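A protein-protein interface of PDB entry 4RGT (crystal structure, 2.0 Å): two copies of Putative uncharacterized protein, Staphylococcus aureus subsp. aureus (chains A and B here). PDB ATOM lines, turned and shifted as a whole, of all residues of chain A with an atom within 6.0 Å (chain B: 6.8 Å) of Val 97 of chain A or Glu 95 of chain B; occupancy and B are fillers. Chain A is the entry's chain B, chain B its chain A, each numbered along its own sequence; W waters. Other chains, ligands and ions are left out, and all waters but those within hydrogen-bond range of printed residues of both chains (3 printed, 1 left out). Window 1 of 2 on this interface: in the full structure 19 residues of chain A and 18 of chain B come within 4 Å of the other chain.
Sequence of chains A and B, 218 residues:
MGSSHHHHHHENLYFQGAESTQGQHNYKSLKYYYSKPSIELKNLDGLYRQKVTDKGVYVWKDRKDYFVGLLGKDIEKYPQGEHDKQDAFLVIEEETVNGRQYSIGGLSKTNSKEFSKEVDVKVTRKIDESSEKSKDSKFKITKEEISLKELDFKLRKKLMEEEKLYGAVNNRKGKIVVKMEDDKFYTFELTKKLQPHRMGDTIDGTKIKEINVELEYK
Water W2 lies within hydrogen-bond range of OE1 of Glu 95 of chain B (2.8 Å), ND2 of Asn 98 of chain A (2.8 Å) and OD1 of Asp 54 of chain A (3.2 Å).
Water W1 bridges the side-chain amide nitrogen of Asn 98 of chain B and the side-chain carboxylate of Glu 95 of chain A.
Water W3 lies within hydrogen-bond range of N of Gly 99 of chain B (3.1 Å), OG1 of Thr 96 of chain A (3.1 Å), N of Gly 99 of chain A (3.1 Å) and OG1 of Thr 96 of chain B (3.5 Å).
Glu 95 of chain A touches Val 97 of chain B, and with the chains exchanged Val 97 of chain A touches Glu 95 of chain B.
Glu 95 of chain A touches Asn 98 of chain B, and with the chains exchanged Asn 98 of chain A touches Glu 95 of chain B.
Thr 96 of chain A touches Val 97 of chain B, and with the chains exchanged Val 97 of chain A touches Thr 96 of chain B.
Thr 96 of chain A touches Asn 98 of chain B, and with the chains exchanged Asn 98 of chain A touches Thr 96 of chain B.
Of the 14 pairs that touch across the chains among the printed residues, 8 have their exchanged pair printed and touching as well.
O of Asn 98 of chain B sits at hydrogen-bond distance from NH1 of Arg 100 of chain B, 3.0 Å away.
The backbone carbonyl oxygen of Tyr 102 of chain B lies within hydrogen-bond range of the backbone NH of Glu 93 of chain B (2.8 Å).
N of Phe 67 of chain A lies within hydrogen-bond range of O of Gln 101 of chain A, at 2.9 Å.
The side-chain carboxylate of Glu 94 of chain B is in salt-bridge range of the side-chain amino group of Lys 36 of chain B (2.7 Å).
O of Asn 98 of chain A lies within hydrogen-bond range of NH1 of Arg 100 of chain A (2.7 Å).
Thr 53 of chain A touches Glu 94 of chain B.
OD1 of Asp 54 of chain A touches CB of Glu 94 of chain B, at 3.9 Å.
OE1 of Glu 95 of chain B touches CA of Asp 54 of chain A (3.5 Å).
Glu 95 of chain B touches Phe 67 of chain A (CG to CE2, 3.98 Å).
Val 97 of chain B touches Glu 95 of chain A.
OD1 of Asn 98 of chain B touches CA of Glu 95 of chain A, at 3.4 Å.
O of Thr 96 of chain A touches CA of Val 97 of chain B, at 3.4 Å.
CG1 of Val 97 of chain A touches CB of Glu 95 of chain B, at 3.8 Å.
CA of Val 97 of chain A touches O of Thr 96 of chain B, at 3.4 Å.
CA of Glu 95 of chain B touches OD1 of Asn 98 of chain A, 3.5 Å away.
Of the printed residues of chain B, Thr 53 of chain A touches Glu 94 (3.3 Å).
Of the printed residues of chain B, Asp 54 of chain A touches Glu 94 and Glu 95.
Of the printed residues of chain B, Thr 96 of chain A touches Val 97 and Asn 98.
Of chain B, only Glu 95 and Thr 96 come within 4 Å of Val 97 of chain A.
Of the printed residues of chain A, Glu 95 of chain B touches Asp 54, Lys 55, Phe 67, Val 97 and Asn 98.
Of the 13 printed residues of chain B, 6 touch a printed residue of chain A.
Hydrophobic or aromatic side chains of chain B within 4 Å of the printed part of chain A: Val 97.
Hydrophobic or aromatic side chains of chain A within 4 Å of the printed part of chain B: Phe 67 and Val 97.
Among the printed residues, 14 pairs touch across the chains.
Among the printed residues, Asp or Glu carboxylates within 4 Å of a Lys or Arg side-chain nitrogen of the other chain: Lys 55 of chain A with Glu 93 of chain B (2.6 Å).
O of Thr 96 of chain A is in hydrogen-bond range of N of Asn 98 of chain B, at 2.8 Å.
The backbone NH (N) of Lys 55 of chain A lies within hydrogen-bond range of the side-chain carboxylate (OE1) of Glu 95 of chain B, 2.7 Å away.
The side-chain carboxylate of Glu 93 of chain B is in salt-bridge range of the side-chain amino group of Lys 55 of chain A, at 2.6 Å.
The backbone carbonyl oxygen of Thr 96 of chain B lies within hydrogen-bond range of the backbone NH of Asn 98 of chain A (2.8 Å).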
ATOM      1  N   THR A  53       5.440   6.210 -24.094  1.00  0.00           N
ATOM      2  CA  THR A  53       4.365   6.853 -23.342  1.00  0.00           C
ATOM      3  C   THR A  53       4.827   7.365 -21.968  1.00  0.00           C
ATOM      4  O   THR A  53       4.105   8.116 -21.317  1.00  0.00           O
ATOM      5  CB  THR A  53       3.161   5.919 -23.185  1.00  0.00           C
ATOM      6  OG1 THR A  53       3.605   4.651 -22.698  1.00  0.00           O
ATOM      7  CG2 THR A  53       2.461   5.734 -24.530  1.00  0.00           C
ATOM      8  N   ASP A  54       6.009   6.941 -21.526  1.00  0.00           N
ATOM      9  CA  ASP A  54       6.594   7.408 -20.263  1.00  0.00           C
ATOM     10  C   ASP A  54       7.078   8.863 -20.408  1.00  0.00           C
ATOM     11  O   ASP A  54       7.370   9.299 -21.511  1.00  0.00           O
ATOM     12  CB  ASP A  54       7.828   6.564 -19.868  1.00  0.00           C
ATOM     13  CG  ASP A  54       7.482   5.149 -19.360  1.00  0.00           C
ATOM     14  OD1 ASP A  54       6.299   4.833 -19.053  1.00  0.00           O
ATOM     15  OD2 ASP A  54       8.435   4.345 -19.241  1.00  0.00           O
ATOM     16  N   LYS A  55       7.171   9.586 -19.287  1.00  0.00           N
ATOM     17  CA  LYS A  55       7.704  10.951 -19.240  1.00  0.00           C
ATOM     18  C   LYS A  55       9.041  10.980 -18.488  1.00  0.00           C
ATOM     19  O   LYS A  55       9.323  11.913 -17.708  1.00  0.00           O
ATOM     20  CB  LYS A  55       6.727  11.913 -18.550  1.00  0.00           C
ATOM     21  CG  LYS A  55       5.431  12.098 -19.293  1.00  0.00           C
ATOM     22  CD  LYS A  55       4.548  13.158 -18.628  1.00  0.00           C
ATOM     23  CE  LYS A  55       3.262  13.302 -19.400  1.00  0.00           C
ATOM     24  NZ  LYS A  55       2.321  14.272 -18.772  1.00  0.00           N
ATOM     25  N   GLY A  56       9.866   9.960 -18.705  1.00  0.00           N
ATOM     26  CA  GLY A  56      11.176   9.945 -18.099  1.00  0.00           C
ATOM     27  C   GLY A  56      11.953   8.690 -18.431  1.00  0.00           C
ATOM     28  O   GLY A  56      11.490   7.817 -19.174  1.00  0.00           O
ATOM     29  N   PHE A  67      14.923   7.875 -11.335  1.00  0.00           N
ATOM     30  CA  PHE A  67      14.010   8.070 -12.456  1.00  0.00           C
ATOM     31  C   PHE A  67      14.118   9.563 -12.757  1.00  0.00           C
ATOM     32  O   PHE A  67      14.008  10.409 -11.837  1.00  0.00           O
ATOM     33  CB  PHE A  67      12.571   7.639 -12.164  1.00  0.00           C
ATOM     34  CG  PHE A  67      11.665   7.723 -13.358  1.00  0.00           C
ATOM     35  CD1 PHE A  67      11.699   6.743 -14.327  1.00  0.00           C
ATOM     36  CD2 PHE A  67      10.787   8.798 -13.531  1.00  0.00           C
ATOM     37  CE1 PHE A  67      10.888   6.810 -15.455  1.00  0.00           C
ATOM     38  CE2 PHE A  67       9.954   8.869 -14.648  1.00  0.00           C
ATOM     39  CZ  PHE A  67      10.010   7.870 -15.616  1.00  0.00           C
ATOM     40  N   GLU A  95       8.992  14.376  -4.385  1.00  0.00           N
ATOM     41  CA  GLU A  95       8.190  13.270  -4.872  1.00  0.00           C
ATOM     42  C   GLU A  95       8.962  12.014  -5.213  1.00  0.00           C
ATOM     43  O   GLU A  95      10.017  12.109  -5.841  1.00  0.00           O
ATOM     44  CB  GLU A  95       7.483  13.691  -6.177  1.00  0.00           C
ATOM     45  CG  GLU A  95       6.389  14.737  -5.999  1.00  0.00           C
ATOM     46  CD  GLU A  95       6.899  16.104  -5.552  1.00  0.00           C
ATOM     47  OE1 GLU A  95       6.237  16.734  -4.689  1.00  0.00           O
ATOM     48  OE2 GLU A  95       7.944  16.557  -6.037  1.00  0.00           O
ATOM     49  N   THR A  96       8.480  10.836  -4.797  1.00  0.00           N
ATOM     50  CA  THR A  96       9.092   9.613  -5.343  1.00  0.00           C
ATOM     51  C   THR A  96       8.295   9.379  -6.618  1.00  0.00           C
ATOM     52  O   THR A  96       7.092   9.698  -6.670  1.00  0.00           O
ATOM     53  CB  THR A  96       8.974   8.346  -4.458  1.00  0.00           C
ATOM     54  OG1 THR A  96       7.614   7.891  -4.463  1.00  0.00           O
ATOM     55  CG2 THR A  96       9.458   8.616  -3.057  1.00  0.00           C
ATOM     56  N   VAL A  97       8.953   8.874  -7.650  1.00  0.00           N
ATOM     57  CA  VAL A  97       8.285   8.554  -8.918  1.00  0.00           C
ATOM     58  C   VAL A  97       8.718   7.164  -9.375  1.00  0.00           C
ATOM     59  O   VAL A  97       9.918   6.842  -9.407  1.00  0.00           O
ATOM     60  CB  VAL A  97       8.540   9.590 -10.028  1.00  0.00           C
ATOM     61  CG1 VAL A  97       7.799   9.198 -11.299  1.00  0.00           C
ATOM     62  CG2 VAL A  97       8.111  10.976  -9.586  1.00  0.00           C
ATOM     63  N   ASN A  98       7.735   6.336  -9.701  1.00  0.00           N
ATOM     64  CA  ASN A  98       7.999   4.946 -10.090  1.00  0.00           C
ATOM     65  C   ASN A  98       8.849   4.208  -9.050  1.00  0.00           C
ATOM     66  O   ASN A  98       9.755   3.434  -9.387  1.00  0.00           O
ATOM     67  CB  ASN A  98       8.617   4.889 -11.489  1.00  0.00           C
ATOM     68  CG  ASN A  98       7.604   5.187 -12.565  1.00  0.00           C
ATOM     69  OD1 ASN A  98       6.386   5.139 -12.327  1.00  0.00           O
ATOM     70  ND2 ASN A  98       8.084   5.525 -13.735  1.00  0.00           N
ATOM     71  N   GLY A  99       8.535   4.471  -7.781  1.00  0.00           N
ATOM     72  CA  GLY A  99       9.236   3.860  -6.654  1.00  0.00           C
ATOM     73  C   GLY A  99      10.692   4.237  -6.542  1.00  0.00           C
ATOM     74  O   GLY A  99      11.459   3.577  -5.839  1.00  0.00           O
ATOM     75  N   ARG A 100      11.091   5.301  -7.219  1.00  0.00           N
ATOM     76  CA  ARG A 100      12.472   5.706  -7.210  1.00  0.00           C
ATOM     77  C   ARG A 100      12.651   7.129  -6.814  1.00  0.00           C
ATOM     78  O   ARG A 100      11.692   7.925  -6.826  1.00  0.00           O
ATOM     79  CB  ARG A 100      13.035   5.519  -8.629  1.00  0.00           C
ATOM     80  CG  ARG A 100      13.229   4.055  -8.959  1.00  0.00           C
ATOM     81  CD  ARG A 100      13.395   3.804 -10.429  1.00  0.00           C
ATOM     82  NE  ARG A 100      13.725   2.404 -10.670  1.00  0.00           N
ATOM     83  CZ  ARG A 100      12.850   1.402 -10.634  1.00  0.00           C
ATOM     84  NH1 ARG A 100      11.576   1.619 -10.339  1.00  0.00           N
ATOM     85  NH2 ARG A 100      13.263   0.168 -10.878  1.00  0.00           N
ATOM     86  N   GLN A 101      13.891   7.470  -6.486  1.00  0.00           N
ATOM     87  CA  GLN A 101      14.241   8.854  -6.241  1.00  0.00           C
ATOM     88  C   GLN A 101      14.093   9.540  -7.606  1.00  0.00           C
ATOM     89  O   GLN A 101      14.359   8.926  -8.644  1.00  0.00           O
ATOM     90  CB  GLN A 101      15.654   8.977  -5.678  1.00  0.00           C
ATOM     91  CG  GLN A 101      15.797   8.405  -4.276  1.00  0.00           C
ATOM     92  CD  GLN A 101      17.205   8.554  -3.720  1.00  0.00           C
ATOM     93  OE1 GLN A 101      17.397   9.120  -2.649  1.00  0.00           O
ATOM     94  NE2 GLN A 101      18.191   8.075  -4.459  1.00  0.00           N
ATOM     95  N   TYR A 102      13.698  10.810  -7.612  1.00  0.00           N
ATOM     96  CA  TYR A 102      13.368  11.498  -8.868  1.00  0.00           C
ATOM     97  C   TYR A 102      14.080  12.817  -9.020  1.00  0.00           C
ATOM     98  O   TYR A 102      14.359  13.512  -8.027  1.00  0.00           O
ATOM     99  CB  TYR A 102      11.833  11.720  -8.868  1.00  0.00           C
ATOM    100  CG  TYR A 102      11.182  12.434 -10.055  1.00  0.00           C
ATOM    101  CD1 TYR A 102      11.167  11.870 -11.334  1.00  0.00           C
ATOM    102  CD2 TYR A 102      10.444  13.596  -9.853  1.00  0.00           C
ATOM    103  CE1 TYR A 102      10.502  12.513 -12.400  1.00  0.00           C
ATOM    104  CE2 TYR A 102       9.776  14.232 -10.888  1.00  0.00           C
ATOM    105  CZ  TYR A 102       9.809  13.689 -12.174  1.00  0.00           C
ATOM    106  OH  TYR A 102       9.151  14.356 -13.206  1.00  0.00           O
ATOM    107  N   LYS B  36      -7.067   8.317 -23.740  1.00  0.00           N
ATOM    108  CA  LYS B  36      -7.277   7.825 -22.392  1.00  0.00           C
ATOM    109  C   LYS B  36      -8.631   8.180 -21.799  1.00  0.00           C
ATOM    110  O   LYS B  36      -9.245   9.180 -22.177  1.00  0.00           O
ATOM    111  CB  LYS B  36      -6.218   8.378 -21.452  1.00  0.00           C
ATOM    112  CG  LYS B  36      -4.890   7.666 -21.515  1.00  0.00           C
ATOM    113  CD  LYS B  36      -3.948   8.222 -20.480  1.00  0.00           C
ATOM    114  CE  LYS B  36      -2.788   7.272 -20.273  1.00  0.00           C
ATOM    115  NZ  LYS B  36      -1.817   7.883 -19.336  1.00  0.00           N
ATOM    116  N   ILE B  92      -5.227   9.703 -15.836  1.00  0.00           N
ATOM    117  CA  ILE B  92      -4.172   8.971 -15.163  1.00  0.00           C
ATOM    118  C   ILE B  92      -2.918   8.819 -16.021  1.00  0.00           C
ATOM    119  O   ILE B  92      -2.960   8.312 -17.147  1.00  0.00           O
ATOM    120  CB  ILE B  92      -4.686   7.612 -14.649  1.00  0.00           C
ATOM    121  CG1 ILE B  92      -5.919   7.829 -13.751  1.00  0.00           C
ATOM    122  CG2 ILE B  92      -3.589   6.877 -13.876  1.00  0.00           C
ATOM    123  CD1 ILE B  92      -5.687   8.732 -12.558  1.00  0.00           C
ATOM    124  N   GLU B  93      -1.813   9.317 -15.481  1.00  0.00           N
ATOM    125  CA  GLU B  93      -0.497   9.297 -16.160  1.00  0.00           C
ATOM    126  C   GLU B  93       0.153   7.910 -16.064  1.00  0.00           C
ATOM    127  O   GLU B  93      -0.329   7.041 -15.344  1.00  0.00           O
ATOM    128  CB  GLU B  93       0.413  10.315 -15.483  1.00  0.00           C
ATOM    129  CG  GLU B  93      -0.094  11.748 -15.536  1.00  0.00           C
ATOM    130  CD  GLU B  93       0.179  12.410 -16.853  1.00  0.00           C
ATOM    131  OE1 GLU B  93       1.332  12.287 -17.335  1.00  0.00           O
ATOM    132  OE2 GLU B  93      -0.718  13.095 -17.391  1.00  0.00           O
ATOM    133  N   GLU B  94       1.262   7.709 -16.787  1.00  0.00           N
ATOM    134  CA  GLU B  94       1.958   6.436 -16.768  1.00  0.00           C
ATOM    135  C   GLU B  94       2.780   6.285 -15.513  1.00  0.00           C
ATOM    136  O   GLU B  94       2.946   5.187 -15.001  1.00  0.00           O
ATOM    137  CB  GLU B  94       2.877   6.294 -17.996  1.00  0.00           C
ATOM    138  CG  GLU B  94       2.106   6.353 -19.300  1.00  0.00           C
ATOM    139  CD  GLU B  94       0.991   5.337 -19.320  1.00  0.00           C
ATOM    140  OE1 GLU B  94      -0.186   5.754 -19.428  1.00  0.00           O
ATOM    141  OE2 GLU B  94       1.288   4.141 -19.143  1.00  0.00           O
ATOM    142  N   GLU B  95       3.297   7.401 -15.020  1.00  0.00           N
ATOM    143  CA  GLU B  95       4.126   7.408 -13.820  1.00  0.00           C
ATOM    144  C   GLU B  95       3.309   7.278 -12.549  1.00  0.00           C
ATOM    145  O   GLU B  95       2.260   7.925 -12.431  1.00  0.00           O
ATOM    146  CB  GLU B  95       4.867   8.745 -13.710  1.00  0.00           C
ATOM    147  CG  GLU B  95       5.973   8.971 -14.715  1.00  0.00           C
ATOM    148  CD  GLU B  95       5.484   9.072 -16.133  1.00  0.00           C
ATOM    149  OE1 GLU B  95       6.141   8.488 -17.004  1.00  0.00           O
ATOM    150  OE2 GLU B  95       4.448   9.725 -16.363  1.00  0.00           O
ATOM    151  N   THR B  96       3.778   6.460 -11.601  1.00  0.00           N
ATOM    152  CA  THR B  96       3.168   6.405 -10.277  1.00  0.00           C
ATOM    153  C   THR B  96       3.953   7.430  -9.470  1.00  0.00           C
ATOM    154  O   THR B  96       5.158   7.537  -9.634  1.00  0.00           O
ATOM    155  CB  THR B  96       3.285   5.028  -9.610  1.00  0.00           C
ATOM    156  OG1 THR B  96       4.661   4.743  -9.320  1.00  0.00           O
ATOM    157  CG2 THR B  96       2.712   3.952 -10.509  1.00  0.00           C
ATOM    158  N   VAL B  97       3.270   8.257  -8.691  1.00  0.00           N
ATOM    159  CA  VAL B  97       3.943   9.274  -7.871  1.00  0.00           C
ATOM    160  C   VAL B  97       3.541   9.156  -6.390  1.00  0.00           C
ATOM    161  O   VAL B  97       2.352   9.059  -6.044  1.00  0.00           O
ATOM    162  CB  VAL B  97       3.671  10.690  -8.385  1.00  0.00           C
ATOM    163  CG1 VAL B  97       4.436  11.700  -7.556  1.00  0.00           C
ATOM    164  CG2 VAL B  97       4.096  10.804  -9.835  1.00  0.00           C
ATOM    165  N   ASN B  98       4.538   9.204  -5.513  1.00  0.00           N
ATOM    166  CA  ASN B  98       4.313   9.014  -4.072  1.00  0.00           C
ATOM    167  C   ASN B  98       3.489   7.752  -3.805  1.00  0.00           C
ATOM    168  O   ASN B  98       2.641   7.694  -2.890  1.00  0.00           O
ATOM    169  CB  ASN B  98       3.731  10.276  -3.418  1.00  0.00           C
ATOM    170  CG  ASN B  98       4.754  11.399  -3.326  1.00  0.00           C
ATOM    171  OD1 ASN B  98       5.963  11.165  -3.417  1.00  0.00           O
ATOM    172  ND2 ASN B  98       4.284  12.622  -3.153  1.00  0.00           N
ATOM    173  N   GLY B  99       3.773   6.720  -4.605  1.00  0.00           N
ATOM    174  CA  GLY B  99       3.106   5.421  -4.474  1.00  0.00           C
ATOM    175  C   GLY B  99       1.649   5.380  -4.893  1.00  0.00           C
ATOM    176  O   GLY B  99       0.970   4.404  -4.640  1.00  0.00           O
ATOM    177  N   ARG B 100       1.178   6.415  -5.574  1.00  0.00           N
ATOM    178  CA  ARG B 100      -0.217   6.487  -6.003  1.00  0.00           C
ATOM    179  C   ARG B 100      -0.397   6.785  -7.489  1.00  0.00           C
ATOM    180  O   ARG B 100       0.543   7.223  -8.182  1.00  0.00           O
ATOM    181  CB  ARG B 100      -0.895   7.611  -5.213  1.00  0.00           C
ATOM    182  CG  ARG B 100      -1.026   7.306  -3.720  1.00  0.00           C
ATOM    183  CD  ARG B 100      -1.318   8.562  -2.921  1.00  0.00           C
ATOM    184  NE  ARG B 100      -1.638   8.257  -1.527  1.00  0.00           N
ATOM    185  CZ  ARG B 100      -0.753   8.004  -0.564  1.00  0.00           C
ATOM    186  NH1 ARG B 100       0.545   7.986  -0.806  1.00  0.00           N
ATOM    187  NH2 ARG B 100      -1.189   7.746   0.668  1.00  0.00           N
ATOM    188  N   GLN B 101      -1.605   6.546  -7.983  1.00  0.00           N
ATOM    189  CA  GLN B 101      -1.943   6.948  -9.346  1.00  0.00           C
ATOM    190  C   GLN B 101      -1.851   8.484  -9.392  1.00  0.00           C
ATOM    191  O   GLN B 101      -2.241   9.178  -8.446  1.00  0.00           O
ATOM    192  CB  GLN B 101      -3.323   6.454  -9.756  1.00  0.00           C
ATOM    193  CG  GLN B 101      -3.387   4.944  -9.921  1.00  0.00           C
ATOM    194  CD  GLN B 101      -4.676   4.471 -10.577  1.00  0.00           C
ATOM    195  OE1 GLN B 101      -4.645   3.875 -11.647  1.00  0.00           O
ATOM    196  NE2 GLN B 101      -5.808   4.767  -9.963  1.00  0.00           N
ATOM    197  N   TYR B 102      -1.395   8.994 -10.525  1.00  0.00           N
ATOM    198  CA  TYR B 102      -1.069  10.413 -10.707  1.00  0.00           C
ATOM    199  C   TYR B 102      -1.769  11.072 -11.875  1.00  0.00           C
ATOM    200  O   TYR B 102      -2.009  10.447 -12.920  1.00  0.00           O
ATOM    201  CB  TYR B 102       0.450  10.464 -10.972  1.00  0.00           C
ATOM    202  CG  TYR B 102       1.103  11.816 -11.163  1.00  0.00           C
ATOM    203  CD1 TYR B 102       1.143  12.736 -10.135  1.00  0.00           C
ATOM    204  CD2 TYR B 102       1.790  12.123 -12.339  1.00  0.00           C
ATOM    205  CE1 TYR B 102       1.797  13.942 -10.297  1.00  0.00           C
ATOM    206  CE2 TYR B 102       2.456  13.322 -12.501  1.00  0.00           C
ATOM    207  CZ  TYR B 102       2.448  14.230 -11.467  1.00  0.00           C
ATOM    208  OH  TYR B 102       3.098  15.439 -11.585  1.00  0.00           O
ATOM    209  N   SER B 103      -2.093  12.345 -11.678  1.00  0.00           N
ATOM    210  CA  SER B 103      -2.696  13.158 -12.704  1.00  0.00           C
ATOM    211  C   SER B 103      -2.139  14.543 -12.502  1.00  0.00           C
ATOM    212  O   SER B 103      -1.673  14.889 -11.386  1.00  0.00           O
ATOM    213  CB  SER B 103      -4.208  13.133 -12.613  1.00  0.00           C
ATOM    214  OG  SER B 103      -4.790  13.883 -13.679  1.00  0.00           O
HETATM  215  O   HOH W   1       5.782  14.877  -2.560  1.00  0.00           O
HETATM  216  O   HOH W   2       6.596   5.921 -16.076  1.00  0.00           O
HETATM  217  O   HOH W   3       6.124   5.979  -6.442  1.00  0.00           O
